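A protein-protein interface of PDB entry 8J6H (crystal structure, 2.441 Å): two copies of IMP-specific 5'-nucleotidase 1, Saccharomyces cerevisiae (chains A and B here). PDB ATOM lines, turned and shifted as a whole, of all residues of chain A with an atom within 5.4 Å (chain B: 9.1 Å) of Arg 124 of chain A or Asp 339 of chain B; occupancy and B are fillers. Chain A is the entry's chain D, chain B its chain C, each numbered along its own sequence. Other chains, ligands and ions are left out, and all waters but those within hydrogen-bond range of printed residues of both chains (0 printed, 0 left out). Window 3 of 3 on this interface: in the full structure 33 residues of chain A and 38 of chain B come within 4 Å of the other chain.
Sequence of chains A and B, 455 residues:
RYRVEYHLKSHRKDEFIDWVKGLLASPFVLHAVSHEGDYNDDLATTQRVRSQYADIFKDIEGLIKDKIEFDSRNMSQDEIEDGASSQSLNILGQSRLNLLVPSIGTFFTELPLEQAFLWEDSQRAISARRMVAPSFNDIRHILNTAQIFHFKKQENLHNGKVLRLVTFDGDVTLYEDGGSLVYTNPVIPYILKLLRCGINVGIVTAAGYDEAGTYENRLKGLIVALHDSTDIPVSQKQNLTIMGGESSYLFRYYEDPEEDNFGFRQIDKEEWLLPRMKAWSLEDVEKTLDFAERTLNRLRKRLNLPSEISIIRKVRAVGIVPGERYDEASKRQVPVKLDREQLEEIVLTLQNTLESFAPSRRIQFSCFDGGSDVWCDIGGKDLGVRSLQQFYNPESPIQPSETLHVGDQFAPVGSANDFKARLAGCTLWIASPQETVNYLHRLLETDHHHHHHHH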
ATOM      1  N   GLU A 120      18.757  24.311  17.442  1.00  0.00           N
ATOM      2  CA  GLU A 120      18.405  23.721  16.151  1.00  0.00           C
ATOM      3  C   GLU A 120      18.949  24.551  14.993  1.00  0.00           C
ATOM      4  O   GLU A 120      19.221  24.024  13.915  1.00  0.00           O
ATOM      5  CB  GLU A 120      16.887  23.576  16.015  1.00  0.00           C
ATOM      6  CG  GLU A 120      16.256  22.587  16.984  1.00  0.00           C
ATOM      7  CD  GLU A 120      16.352  21.149  16.507  1.00  0.00           C
ATOM      8  OE1 GLU A 120      16.948  20.910  15.435  1.00  0.00           O
ATOM      9  OE2 GLU A 120      15.836  20.255  17.210  1.00  0.00           O
ATOM     10  N   ASP A 121      19.100  25.852  15.222  1.00  0.00           N
ATOM     11  CA  ASP A 121      19.645  26.749  14.209  1.00  0.00           C
ATOM     12  C   ASP A 121      21.099  26.398  13.912  1.00  0.00           C
ATOM     13  O   ASP A 121      21.591  26.625  12.809  1.00  0.00           O
ATOM     14  CB  ASP A 121      19.532  28.205  14.663  1.00  0.00           C
ATOM     15  CG  ASP A 121      19.890  29.186  13.568  1.00  0.00           C
ATOM     16  OD1 ASP A 121      19.700  28.850  12.380  1.00  0.00           O
ATOM     17  OD2 ASP A 121      20.360  30.296  13.895  1.00  0.00           O
ATOM     18  N   SER A 122      21.783  25.848  14.907  1.00  0.00           N
ATOM     19  CA  SER A 122      23.145  25.369  14.718  1.00  0.00           C
ATOM     20  C   SER A 122      23.139  24.131  13.830  1.00  0.00           C
ATOM     21  O   SER A 122      23.913  24.029  12.879  1.00  0.00           O
ATOM     22  CB  SER A 122      23.802  25.057  16.063  1.00  0.00           C
ATOM     23  OG  SER A 122      23.169  23.956  16.693  1.00  0.00           O
ATOM     24  N   GLN A 123      22.245  23.199  14.144  1.00  0.00           N
ATOM     25  CA  GLN A 123      22.147  21.946  13.407  1.00  0.00           C
ATOM     26  C   GLN A 123      21.566  22.145  12.011  1.00  0.00           C
ATOM     27  O   GLN A 123      22.170  21.746  11.016  1.00  0.00           O
ATOM     28  CB  GLN A 123      21.287  20.944  14.178  1.00  0.00           C
ATOM     29  CG  GLN A 123      21.462  20.996  15.685  1.00  0.00           C
ATOM     30  CD  GLN A 123      22.853  20.597  16.132  1.00  0.00           C
ATOM     31  OE1 GLN A 123      23.423  19.627  15.635  1.00  0.00           O
ATOM     32  NE2 GLN A 123      23.405  21.344  17.083  1.00  0.00           N
ATOM     33  N   ARG A 124      20.393  22.768  11.943  1.00  0.00           N
ATOM     34  CA  ARG A 124      19.632  22.824  10.700  1.00  0.00           C
ATOM     35  C   ARG A 124      19.924  24.068   9.858  1.00  0.00           C
ATOM     36  O   ARG A 124      19.503  24.145   8.703  1.00  0.00           O
ATOM     37  CB  ARG A 124      18.134  22.746  11.004  1.00  0.00           C
ATOM     38  CG  ARG A 124      17.784  21.789  12.136  1.00  0.00           C
ATOM     39  CD  ARG A 124      16.330  21.357  12.074  1.00  0.00           C
ATOM     40  NE  ARG A 124      16.149  20.183  11.226  1.00  0.00           N
ATOM     41  CZ  ARG A 124      15.022  19.888  10.586  1.00  0.00           C
ATOM     42  NH1 ARG A 124      13.969  20.688  10.689  1.00  0.00           N
ATOM     43  NH2 ARG A 124      14.948  18.795   9.837  1.00  0.00           N
ATOM     44  N   ALA A 125      20.637  25.029  10.441  1.00  0.00           N
ATOM     45  CA  ALA A 125      21.015  26.266   9.750  1.00  0.00           C
ATOM     46  C   ALA A 125      19.806  27.001   9.175  1.00  0.00           C
ATOM     47  O   ALA A 125      19.760  27.306   7.983  1.00  0.00           O
ATOM     48  CB  ALA A 125      22.026  25.969   8.648  1.00  0.00           C
ATOM     49  N   ILE A 126      18.834  27.290  10.034  1.00  0.00           N
ATOM     50  CA  ILE A 126      17.590  27.924   9.612  1.00  0.00           C
ATOM     51  C   ILE A 126      17.786  29.389   9.231  1.00  0.00           C
ATOM     52  O   ILE A 126      17.310  29.837   8.188  1.00  0.00           O
ATOM     53  CB  ILE A 126      16.523  27.839  10.720  1.00  0.00           C
ATOM     54  CG1 ILE A 126      16.466  26.424  11.297  1.00  0.00           C
ATOM     55  CG2 ILE A 126      15.163  28.270  10.188  1.00  0.00           C
ATOM     56  CD1 ILE A 126      15.697  26.322  12.594  1.00  0.00           C
ATOM     57  N   ARG A 129      19.364  30.448   5.744  1.00  0.00           N
ATOM     58  CA  ARG A 129      18.619  30.277   4.501  1.00  0.00           C
ATOM     59  C   ARG A 129      18.038  31.599   4.012  1.00  0.00           C
ATOM     60  O   ARG A 129      17.580  32.422   4.805  1.00  0.00           O
ATOM     61  CB  ARG A 129      17.504  29.245   4.677  1.00  0.00           C
ATOM     62  CG  ARG A 129      17.994  27.878   5.129  1.00  0.00           C
ATOM     63  CD  ARG A 129      17.007  26.786   4.752  1.00  0.00           C
ATOM     64  NE  ARG A 129      15.689  27.009   5.337  1.00  0.00           N
ATOM     65  CZ  ARG A 129      15.265  26.442   6.462  1.00  0.00           C
ATOM     66  NH1 ARG A 129      14.048  26.702   6.920  1.00  0.00           N
ATOM     67  NH2 ARG A 129      16.057  25.612   7.127  1.00  0.00           N
ATOM     68  N   SER A 135      10.482  26.175   8.329  1.00  0.00           N
ATOM     69  CA  SER A 135       9.465  25.196   7.968  1.00  0.00           C
ATOM     70  C   SER A 135       8.681  24.667   9.163  1.00  0.00           C
ATOM     71  O   SER A 135       9.028  24.926  10.316  1.00  0.00           O
ATOM     72  CB  SER A 135      10.111  24.027   7.222  1.00  0.00           C
ATOM     73  OG  SER A 135      10.904  23.242   8.097  1.00  0.00           O
ATOM     74  N   ASN A 137       8.507  21.522   9.981  1.00  0.00           N
ATOM     75  CA  ASN A 137       9.410  20.570  10.617  1.00  0.00           C
ATOM     76  C   ASN A 137      10.444  21.254  11.502  1.00  0.00           C
ATOM     77  O   ASN A 137      10.861  20.701  12.519  1.00  0.00           O
ATOM     78  CB  ASN A 137      10.114  19.716   9.560  1.00  0.00           C
ATOM     79  CG  ASN A 137       9.490  18.342   9.411  1.00  0.00           C
ATOM     80  OD1 ASN A 137       8.374  18.099   9.871  1.00  0.00           O
ATOM     81  ND2 ASN A 137      10.213  17.432   8.769  1.00  0.00           N
ATOM     82  N   ASP A 138      10.860  22.454  11.107  1.00  0.00           N
ATOM     83  CA  ASP A 138      11.783  23.242  11.915  1.00  0.00           C
ATOM     84  C   ASP A 138      11.162  23.566  13.266  1.00  0.00           C
ATOM     85  O   ASP A 138      11.766  23.316  14.310  1.00  0.00           O
ATOM     86  CB  ASP A 138      12.177  24.534  11.195  1.00  0.00           C
ATOM     87  CG  ASP A 138      13.107  24.288  10.023  1.00  0.00           C
ATOM     88  OD1 ASP A 138      13.809  23.255  10.027  1.00  0.00           O
ATOM     89  OD2 ASP A 138      13.140  25.132   9.102  1.00  0.00           O
ATOM     90  N   HIS A 141      10.707  20.495  15.394  1.00  0.00           N
ATOM     91  CA  HIS A 141      11.980  20.132  16.006  1.00  0.00           C
ATOM     92  C   HIS A 141      12.290  21.031  17.197  1.00  0.00           C
ATOM     93  O   HIS A 141      12.742  20.561  18.241  1.00  0.00           O
ATOM     94  CB  HIS A 141      13.113  20.210  14.981  1.00  0.00           C
ATOM     95  CG  HIS A 141      13.257  18.979  14.142  1.00  0.00           C
ATOM     96  ND1 HIS A 141      12.349  18.633  13.164  1.00  0.00           N
ATOM     97  CD2 HIS A 141      14.202  18.009  14.136  1.00  0.00           C
ATOM     98  CE1 HIS A 141      12.730  17.505  12.591  1.00  0.00           C
ATOM     99  NE2 HIS A 141      13.851  17.106  13.163  1.00  0.00           N
ATOM    100  N   ARG B 302      27.926  29.676   4.004  1.00  0.00           N
ATOM    101  CA  ARG B 302      26.819  30.397   4.626  1.00  0.00           C
ATOM    102  C   ARG B 302      25.960  29.472   5.481  1.00  0.00           C
ATOM    103  O   ARG B 302      25.577  29.824   6.597  1.00  0.00           O
ATOM    104  CB  ARG B 302      25.955  31.084   3.563  1.00  0.00           C
ATOM    105  CG  ARG B 302      24.597  31.542   4.079  1.00  0.00           C
ATOM    106  CD  ARG B 302      24.060  32.728   3.295  1.00  0.00           C
ATOM    107  NE  ARG B 302      24.078  32.497   1.854  1.00  0.00           N
ATOM    108  CZ  ARG B 302      23.135  31.839   1.189  1.00  0.00           C
ATOM    109  NH1 ARG B 302      22.091  31.336   1.836  1.00  0.00           N
ATOM    110  NH2 ARG B 302      23.237  31.682  -0.124  1.00  0.00           N
ATOM    111  N   LEU B 303      25.667  28.285   4.959  1.00  0.00           N
ATOM    112  CA  LEU B 303      24.870  27.306   5.692  1.00  0.00           C
ATOM    113  C   LEU B 303      25.718  26.547   6.708  1.00  0.00           C
ATOM    114  O   LEU B 303      25.187  25.798   7.528  1.00  0.00           O
ATOM    115  CB  LEU B 303      24.205  26.324   4.726  1.00  0.00           C
ATOM    116  CG  LEU B 303      23.138  26.903   3.795  1.00  0.00           C
ATOM    117  CD1 LEU B 303      22.702  25.870   2.769  1.00  0.00           C
ATOM    118  CD2 LEU B 303      21.944  27.403   4.594  1.00  0.00           C
ATOM    119  N   ASN B 304      27.032  26.754   6.644  1.00  0.00           N
ATOM    120  CA  ASN B 304      27.985  26.096   7.536  1.00  0.00           C
ATOM    121  C   ASN B 304      27.805  24.581   7.552  1.00  0.00           C
ATOM    122  O   ASN B 304      27.752  23.960   8.615  1.00  0.00           O
ATOM    123  CB  ASN B 304      27.862  26.655   8.956  1.00  0.00           C
ATOM    124  CG  ASN B 304      29.097  26.389   9.796  1.00  0.00           C
ATOM    125  OD1 ASN B 304      30.218  26.380   9.287  1.00  0.00           O
ATOM    126  ND2 ASN B 304      28.898  26.169  11.090  1.00  0.00           N
ATOM    127  N   LEU B 305      27.703  23.995   6.363  1.00  0.00           N
ATOM    128  CA  LEU B 305      27.512  22.556   6.222  1.00  0.00           C
ATOM    129  C   LEU B 305      28.719  21.791   6.757  1.00  0.00           C
ATOM    130  O   LEU B 305      29.842  22.294   6.714  1.00  0.00           O
ATOM    131  CB  LEU B 305      27.264  22.196   4.754  1.00  0.00           C
ATOM    132  CG  LEU B 305      26.081  22.886   4.071  1.00  0.00           C
ATOM    133  CD1 LEU B 305      25.934  22.409   2.633  1.00  0.00           C
ATOM    134  CD2 LEU B 305      24.794  22.656   4.851  1.00  0.00           C
ATOM    135  N   PRO B 306      28.487  20.571   7.275  1.00  0.00           N
ATOM    136  CA  PRO B 306      29.573  19.704   7.746  1.00  0.00           C
ATOM    137  C   PRO B 306      30.608  19.464   6.651  1.00  0.00           C
ATOM    138  O   PRO B 306      30.247  19.435   5.476  1.00  0.00           O
ATOM    139  CB  PRO B 306      28.852  18.406   8.116  1.00  0.00           C
ATOM    140  CG  PRO B 306      27.455  18.825   8.420  1.00  0.00           C
ATOM    141  CD  PRO B 306      27.163  19.957   7.481  1.00  0.00           C
ATOM    142  N   ILE B 309      30.331  16.775   3.989  1.00  0.00           N
ATOM    143  CA  ILE B 309      29.594  17.105   2.777  1.00  0.00           C
ATOM    144  C   ILE B 309      30.574  17.547   1.699  1.00  0.00           C
ATOM    145  O   ILE B 309      31.338  18.490   1.893  1.00  0.00           O
ATOM    146  CB  ILE B 309      28.558  18.218   3.019  1.00  0.00           C
ATOM    147  CG1 ILE B 309      27.567  17.797   4.106  1.00  0.00           C
ATOM    148  CG2 ILE B 309      27.827  18.550   1.731  1.00  0.00           C
ATOM    149  CD1 ILE B 309      26.834  16.513   3.795  1.00  0.00           C
ATOM    150  N   ILE B 320      26.577  18.499  -5.005  1.00  0.00           N
ATOM    151  CA  ILE B 320      26.893  18.333  -3.593  1.00  0.00           C
ATOM    152  C   ILE B 320      26.367  16.969  -3.134  1.00  0.00           C
ATOM    153  O   ILE B 320      25.302  16.523  -3.567  1.00  0.00           O
ATOM    154  CB  ILE B 320      26.311  19.499  -2.743  1.00  0.00           C
ATOM    155  CG1 ILE B 320      27.263  19.868  -1.604  1.00  0.00           C
ATOM    156  CG2 ILE B 320      24.904  19.194  -2.236  1.00  0.00           C
ATOM    157  CD1 ILE B 320      26.932  21.190  -0.939  1.00  0.00           C
ATOM    158  N   PRO B 322      26.181  13.656   0.078  1.00  0.00           N
ATOM    159  CA  PRO B 322      26.243  13.282   1.497  1.00  0.00           C
ATOM    160  C   PRO B 322      27.622  12.766   1.914  1.00  0.00           C
ATOM    161  O   PRO B 322      28.494  12.593   1.063  1.00  0.00           O
ATOM    162  CB  PRO B 322      25.186  12.176   1.616  1.00  0.00           C
ATOM    163  CG  PRO B 322      25.000  11.667   0.225  1.00  0.00           C
ATOM    164  CD  PRO B 322      25.176  12.863  -0.651  1.00  0.00           C
ATOM    165  N   VAL B 336      26.147  11.095   7.524  1.00  0.00           N
ATOM    166  CA  VAL B 336      26.037  12.547   7.428  1.00  0.00           C
ATOM    167  C   VAL B 336      25.229  12.920   6.193  1.00  0.00           C
ATOM    168  O   VAL B 336      25.674  12.718   5.064  1.00  0.00           O
ATOM    169  CB  VAL B 336      27.421  13.224   7.367  1.00  0.00           C
ATOM    170  CG1 VAL B 336      27.271  14.710   7.062  1.00  0.00           C
ATOM    171  CG2 VAL B 336      28.173  13.012   8.670  1.00  0.00           C
ATOM    172  N   LYS B 337      24.037  13.458   6.417  1.00  0.00           N
ATOM    173  CA  LYS B 337      23.127  13.796   5.332  1.00  0.00           C
ATOM    174  C   LYS B 337      22.793  15.283   5.323  1.00  0.00           C
ATOM    175  O   LYS B 337      23.333  16.054   6.114  1.00  0.00           O
ATOM    176  CB  LYS B 337      21.841  12.976   5.448  1.00  0.00           C
ATOM    177  CG  LYS B 337      21.942  11.580   4.863  1.00  0.00           C
ATOM    178  CD  LYS B 337      20.952  10.626   5.518  1.00  0.00           C
ATOM    179  CE  LYS B 337      21.684   9.510   6.251  1.00  0.00           C
ATOM    180  NZ  LYS B 337      20.852   8.879   7.314  1.00  0.00           N
ATOM    181  N   LEU B 338      21.901  15.675   4.420  1.00  0.00           N
ATOM    182  CA  LEU B 338      21.444  17.057   4.339  1.00  0.00           C
ATOM    183  C   LEU B 338      19.935  17.140   4.534  1.00  0.00           C
ATOM    184  O   LEU B 338      19.189  16.287   4.052  1.00  0.00           O
ATOM    185  CB  LEU B 338      21.836  17.679   2.996  1.00  0.00           C
ATOM    186  CG  LEU B 338      23.305  18.064   2.816  1.00  0.00           C
ATOM    187  CD1 LEU B 338      23.541  18.635   1.426  1.00  0.00           C
ATOM    188  CD2 LEU B 338      23.726  19.060   3.887  1.00  0.00           C
ATOM    189  N   ASP B 339      19.491  18.167   5.250  1.00  0.00           N
ATOM    190  CA  ASP B 339      18.066  18.400   5.450  1.00  0.00           C
ATOM    191  C   ASP B 339      17.421  18.860   4.148  1.00  0.00           C
ATOM    192  O   ASP B 339      18.085  19.454   3.298  1.00  0.00           O
ATOM    193  CB  ASP B 339      17.836  19.431   6.555  1.00  0.00           C
ATOM    194  CG  ASP B 339      18.394  18.983   7.893  1.00  0.00           C
ATOM    195  OD1 ASP B 339      18.045  17.870   8.338  1.00  0.00           O
ATOM    196  OD2 ASP B 339      19.183  19.741   8.497  1.00  0.00           O
ATOM    197  N   ARG B 340      16.130  18.581   3.993  1.00  0.00           N
ATOM    198  CA  ARG B 340      15.426  18.915   2.761  1.00  0.00           C
ATOM    199  C   ARG B 340      15.370  20.427   2.544  1.00  0.00           C
ATOM    200  O   ARG B 340      15.384  20.892   1.406  1.00  0.00           O
ATOM    201  CB  ARG B 340      14.011  18.324   2.767  1.00  0.00           C
ATOM    202  CG  ARG B 340      12.899  19.349   2.944  1.00  0.00           C
ATOM    203  CD  ARG B 340      11.571  18.851   2.401  1.00  0.00           C
ATOM    204  NE  ARG B 340      10.506  19.828   2.612  1.00  0.00           N
ATOM    205  CZ  ARG B 340       9.278  19.715   2.118  1.00  0.00           C
ATOM    206  NH1 ARG B 340       8.950  18.665   1.380  1.00  0.00           N
ATOM    207  NH2 ARG B 340       8.376  20.658   2.361  1.00  0.00           N
ATOM    208  N   GLU B 341      15.316  21.188   3.635  1.00  0.00           N
ATOM    209  CA  GLU B 341      15.281  22.642   3.538  1.00  0.00           C
ATOM    210  C   GLU B 341      16.599  23.152   2.974  1.00  0.00           C
ATOM    211  O   GLU B 341      16.631  24.113   2.205  1.00  0.00           O
ATOM    212  CB  GLU B 341      15.004  23.280   4.902  1.00  0.00           C
ATOM    213  CG  GLU B 341      13.631  22.968   5.480  1.00  0.00           C
ATOM    214  CD  GLU B 341      13.606  21.675   6.274  1.00  0.00           C
ATOM    215  OE1 GLU B 341      14.683  21.075   6.469  1.00  0.00           O
ATOM    216  OE2 GLU B 341      12.510  21.265   6.711  1.00  0.00           O
ATOM    217  N   GLN B 342      17.684  22.491   3.361  1.00  0.00           N
ATOM    218  CA  GLN B 342      19.011  22.822   2.865  1.00  0.00           C
ATOM    219  C   GLN B 342      19.142  22.453   1.393  1.00  0.00           C
ATOM    220  O   GLN B 342      19.645  23.239   0.590  1.00  0.00           O
ATOM    221  CB  GLN B 342      20.083  22.111   3.691  1.00  0.00           C
ATOM    222  CG  GLN B 342      20.096  22.521   5.153  1.00  0.00           C
ATOM    223  CD  GLN B 342      21.071  21.709   5.978  1.00  0.00           C
ATOM    224  OE1 GLN B 342      21.233  20.507   5.766  1.00  0.00           O
ATOM    225  NE2 GLN B 342      21.732  22.363   6.925  1.00  0.00           N
ATOM    226  N   LEU B 343      18.686  21.253   1.047  1.00  0.00           N
ATOM    227  CA  LEU B 343      18.687  20.795  -0.339  1.00  0.00           C
ATOM    228  C   LEU B 343      17.857  21.726  -1.216  1.00  0.00           C
ATOM    229  O   LEU B 343      18.259  22.072  -2.327  1.00  0.00           O
ATOM    230  CB  LEU B 343      18.145  19.368  -0.437  1.00  0.00           C
ATOM    231  CG  LEU B 343      18.907  18.274   0.315  1.00  0.00           C
ATOM    232  CD1 LEU B 343      18.055  17.021   0.434  1.00  0.00           C
ATOM    233  CD2 LEU B 343      20.224  17.962  -0.372  1.00  0.00           C
ATOM    234  N   GLU B 344      16.700  22.130  -0.701  1.00  0.00           N
ATOM    235  CA  GLU B 344      15.789  23.001  -1.435  1.00  0.00           C
ATOM    236  C   GLU B 344      16.362  24.406  -1.583  1.00  0.00           C
ATOM    237  O   GLU B 344      16.205  25.039  -2.626  1.00  0.00           O
ATOM    238  CB  GLU B 344      14.430  23.058  -0.737  1.00  0.00           C
ATOM    239  CG  GLU B 344      13.244  23.127  -1.682  1.00  0.00           C
ATOM    240  CD  GLU B 344      11.934  23.346  -0.952  1.00  0.00           C
ATOM    241  OE1 GLU B 344      11.898  23.134   0.278  1.00  0.00           O
ATOM    242  OE2 GLU B 344      10.940  23.723  -1.609  1.00  0.00           O
ATOM    243  N   GLU B 345      17.016  24.889  -0.530  1.00  0.00           N
ATOM    244  CA  GLU B 345      17.687  26.185  -0.568  1.00  0.00           C
ATOM    245  C   GLU B 345      18.750  26.204  -1.658  1.00  0.00           C
ATOM    246  O   GLU B 345      18.883  27.179  -2.397  1.00  0.00           O
ATOM    247  CB  GLU B 345      18.320  26.504   0.790  1.00  0.00           C
ATOM    248  CG  GLU B 345      19.267  27.696   0.782  1.00  0.00           C
ATOM    249  CD  GLU B 345      18.561  29.014   1.029  1.00  0.00           C
ATOM    250  OE1 GLU B 345      17.339  28.996   1.297  1.00  0.00           O
ATOM    251  OE2 GLU B 345      19.227  30.068   0.959  1.00  0.00           O
ATOM    252  N   ILE B 346      19.494  25.107  -1.755  1.00  0.00           N
ATOM    253  CA  ILE B 346      20.579  24.985  -2.720  1.00  0.00           C
ATOM    254  C   ILE B 346      20.071  25.005  -4.161  1.00  0.00           C
ATOM    255  O   ILE B 346      20.572  25.768  -4.988  1.00  0.00           O
ATOM    256  CB  ILE B 346      21.387  23.696  -2.479  1.00  0.00           C
ATOM    257  CG1 ILE B 346      22.190  23.809  -1.183  1.00  0.00           C
ATOM    258  CG2 ILE B 346      22.324  23.426  -3.640  1.00  0.00           C
ATOM    259  CD1 ILE B 346      22.809  22.506  -0.728  1.00  0.00           C
ATOM    260  N   ASP B 369      17.288  17.636  -6.595  1.00  0.00           N
ATOM    261  CA  ASP B 369      17.501  17.425  -5.162  1.00  0.00           C
ATOM    262  C   ASP B 369      16.645  16.298  -4.580  1.00  0.00           C
ATOM    263  O   ASP B 369      16.112  16.423  -3.476  1.00  0.00           O
ATOM    264  CB  ASP B 369      17.239  18.717  -4.382  1.00  0.00           C
ATOM    265  CG  ASP B 369      15.788  19.159  -4.444  1.00  0.00           C
ATOM    266  OD1 ASP B 369      15.260  19.336  -5.560  1.00  0.00           O
ATOM    267  OD2 ASP B 369      15.175  19.330  -3.369  1.00  0.00           O
ATOM    268  N   GLY B 370      16.531  15.196  -5.313  1.00  0.00           N
ATOM    269  CA  GLY B 370      15.758  14.054  -4.854  1.00  0.00           C
ATOM    270  C   GLY B 370      16.302  13.446  -3.576  1.00  0.00           C
ATOM    271  O   GLY B 370      15.714  13.605  -2.507  1.00  0.00           O
ATOM    272  N   GLY B 371      17.432  12.751  -3.682  1.00  0.00           N
ATOM    273  CA  GLY B 371      18.058  12.138  -2.523  1.00  0.00           C
ATOM    274  C   GLY B 371      18.721  13.158  -1.618  1.00  0.00           C
ATOM    275  O   GLY B 371      18.249  14.287  -1.487  1.00  0.00           O
ATOM    276  N   SER B 372      19.821  12.764  -0.985  1.00  0.00           N
ATOM    277  CA  SER B 372      20.572  13.684  -0.139  1.00  0.00           C
ATOM    278  C   SER B 372      21.628  14.413  -0.959  1.00  0.00           C
ATOM    279  O   SER B 372      22.548  15.021  -0.411  1.00  0.00           O
ATOM    280  CB  SER B 372      21.225  12.941   1.029  1.00  0.00           C
ATOM    281  OG  SER B 372      21.835  13.850   1.930  1.00  0.00           O
ATOM    282  N   ASP B 373      21.486  14.348  -2.279  1.00  0.00           N
ATOM    283  CA  ASP B 373      22.432  14.980  -3.186  1.00  0.00           C
ATOM    284  C   ASP B 373      21.751  16.012  -4.077  1.00  0.00           C
ATOM    285  O   ASP B 373      20.600  15.841  -4.482  1.00  0.00           O
ATOM    286  CB  ASP B 373      23.130  13.924  -4.050  1.00  0.00           C
ATOM    287  CG  ASP B 373      22.150  13.032  -4.791  1.00  0.00           C
ATOM    288  OD1 ASP B 373      20.946  13.062  -4.462  1.00  0.00           O
ATOM    289  OD2 ASP B 373      22.584  12.298  -5.703  1.00  0.00           O
ATOM    290  N   VAL B 374      22.468  17.091  -4.372  1.00  0.00           N
ATOM    291  CA  VAL B 374      21.993  18.089  -5.319  1.00  0.00           C
ATOM    292  C   VAL B 374      22.915  18.129  -6.530  1.00  0.00           C
ATOM    293  O   VAL B 374      24.107  18.395  -6.396  1.00  0.00           O
ATOM    294  CB  VAL B 374      21.910  19.490  -4.691  1.00  0.00           C
ATOM    295  CG1 VAL B 374      21.607  20.528  -5.760  1.00  0.00           C
ATOM    296  CG2 VAL B 374      20.856  19.518  -3.599  1.00  0.00           C
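Arg 124 of chain A touches just these residues of chain B: Asp 339 and Gln 342. Asp 339 of chain B touches one residue of chain A. No residue of chain B comes within 4 Å of Asp 138 of chain A. Printed residues of chain A within 4 Å of Glu 341 of chain B: Arg 129 and Ser 135. Of the printed residues of chain B, Ser 135 of chain A touches Glu 341. The nearest residue of chain A that does not touch Asp 339 of chain B is Gln 123 of chain A (4.4 Å). The nearest printed residue of chain B that does not touch Arg 129 of chain A is Leu 303 of chain B (4.01 Å).
CB of Ala 125 of chain A touches O of Leu 303 of chain B, at 3.4 Å. NH2 of Arg 129 of chain A touches CB of Glu 341 of chain B (3.4 Å). Arg 129 of chain A touches Glu 345 of chain B (CB to OE1, 3.4 Å).
The guanidinium group (NH1) of Arg 302 of chain B is in salt-bridge range of the side-chain carboxylate (OE2) of Glu 345 of chain B. The backbone NH (N) of Asp 339 of chain B sits at hydrogen-bond distance from the side-chain amide oxygen (OE1) of Gln 342 of chain B, 3.0 Å away. OD1 of Asp 138 of chain A is in salt-bridge range of NH1 of Arg 124 of chain A (2.7 Å). The guanidinium group (NH1) of Arg 129 of chain A lies within salt-bridge range of the side-chain carboxylate (OD2) of Asp 138 of chain A (2.8 Å). OD2 of Asp 138 of chain A lies within hydrogen-bond range of N of Ser 135 of chain A (3.0 Å).
The guanidinium group of Arg 124 of chain A is in salt-bridge range of the side-chain carboxylate of Asp 339 of chain B (3.6 Å). The side-chain hydroxyl (OG) of Ser 135 of chain A is in hydrogen-bond range of the side-chain carboxylate (OE2) of Glu 341 of chain B. NE2 of Gln 342 of chain B is in hydrogen-bond range of O of Arg 124 of chain A.
Of the 12 printed residues of chain A, 4 touch a printed residue of chain B. Hydrophobic or aromatic side chains of chain A within 4 Å of the printed part of chain B: Ala 125. Along chain A the printed residues that touch a printed residue of chain B span positions 124 to 135. Among the printed residues, 6 pairs touch across the chains.
No position is printed for both chains. Of the 6 pairs that touch across the chains among the printed residues, none has its exchanged pair printed and touching as well.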
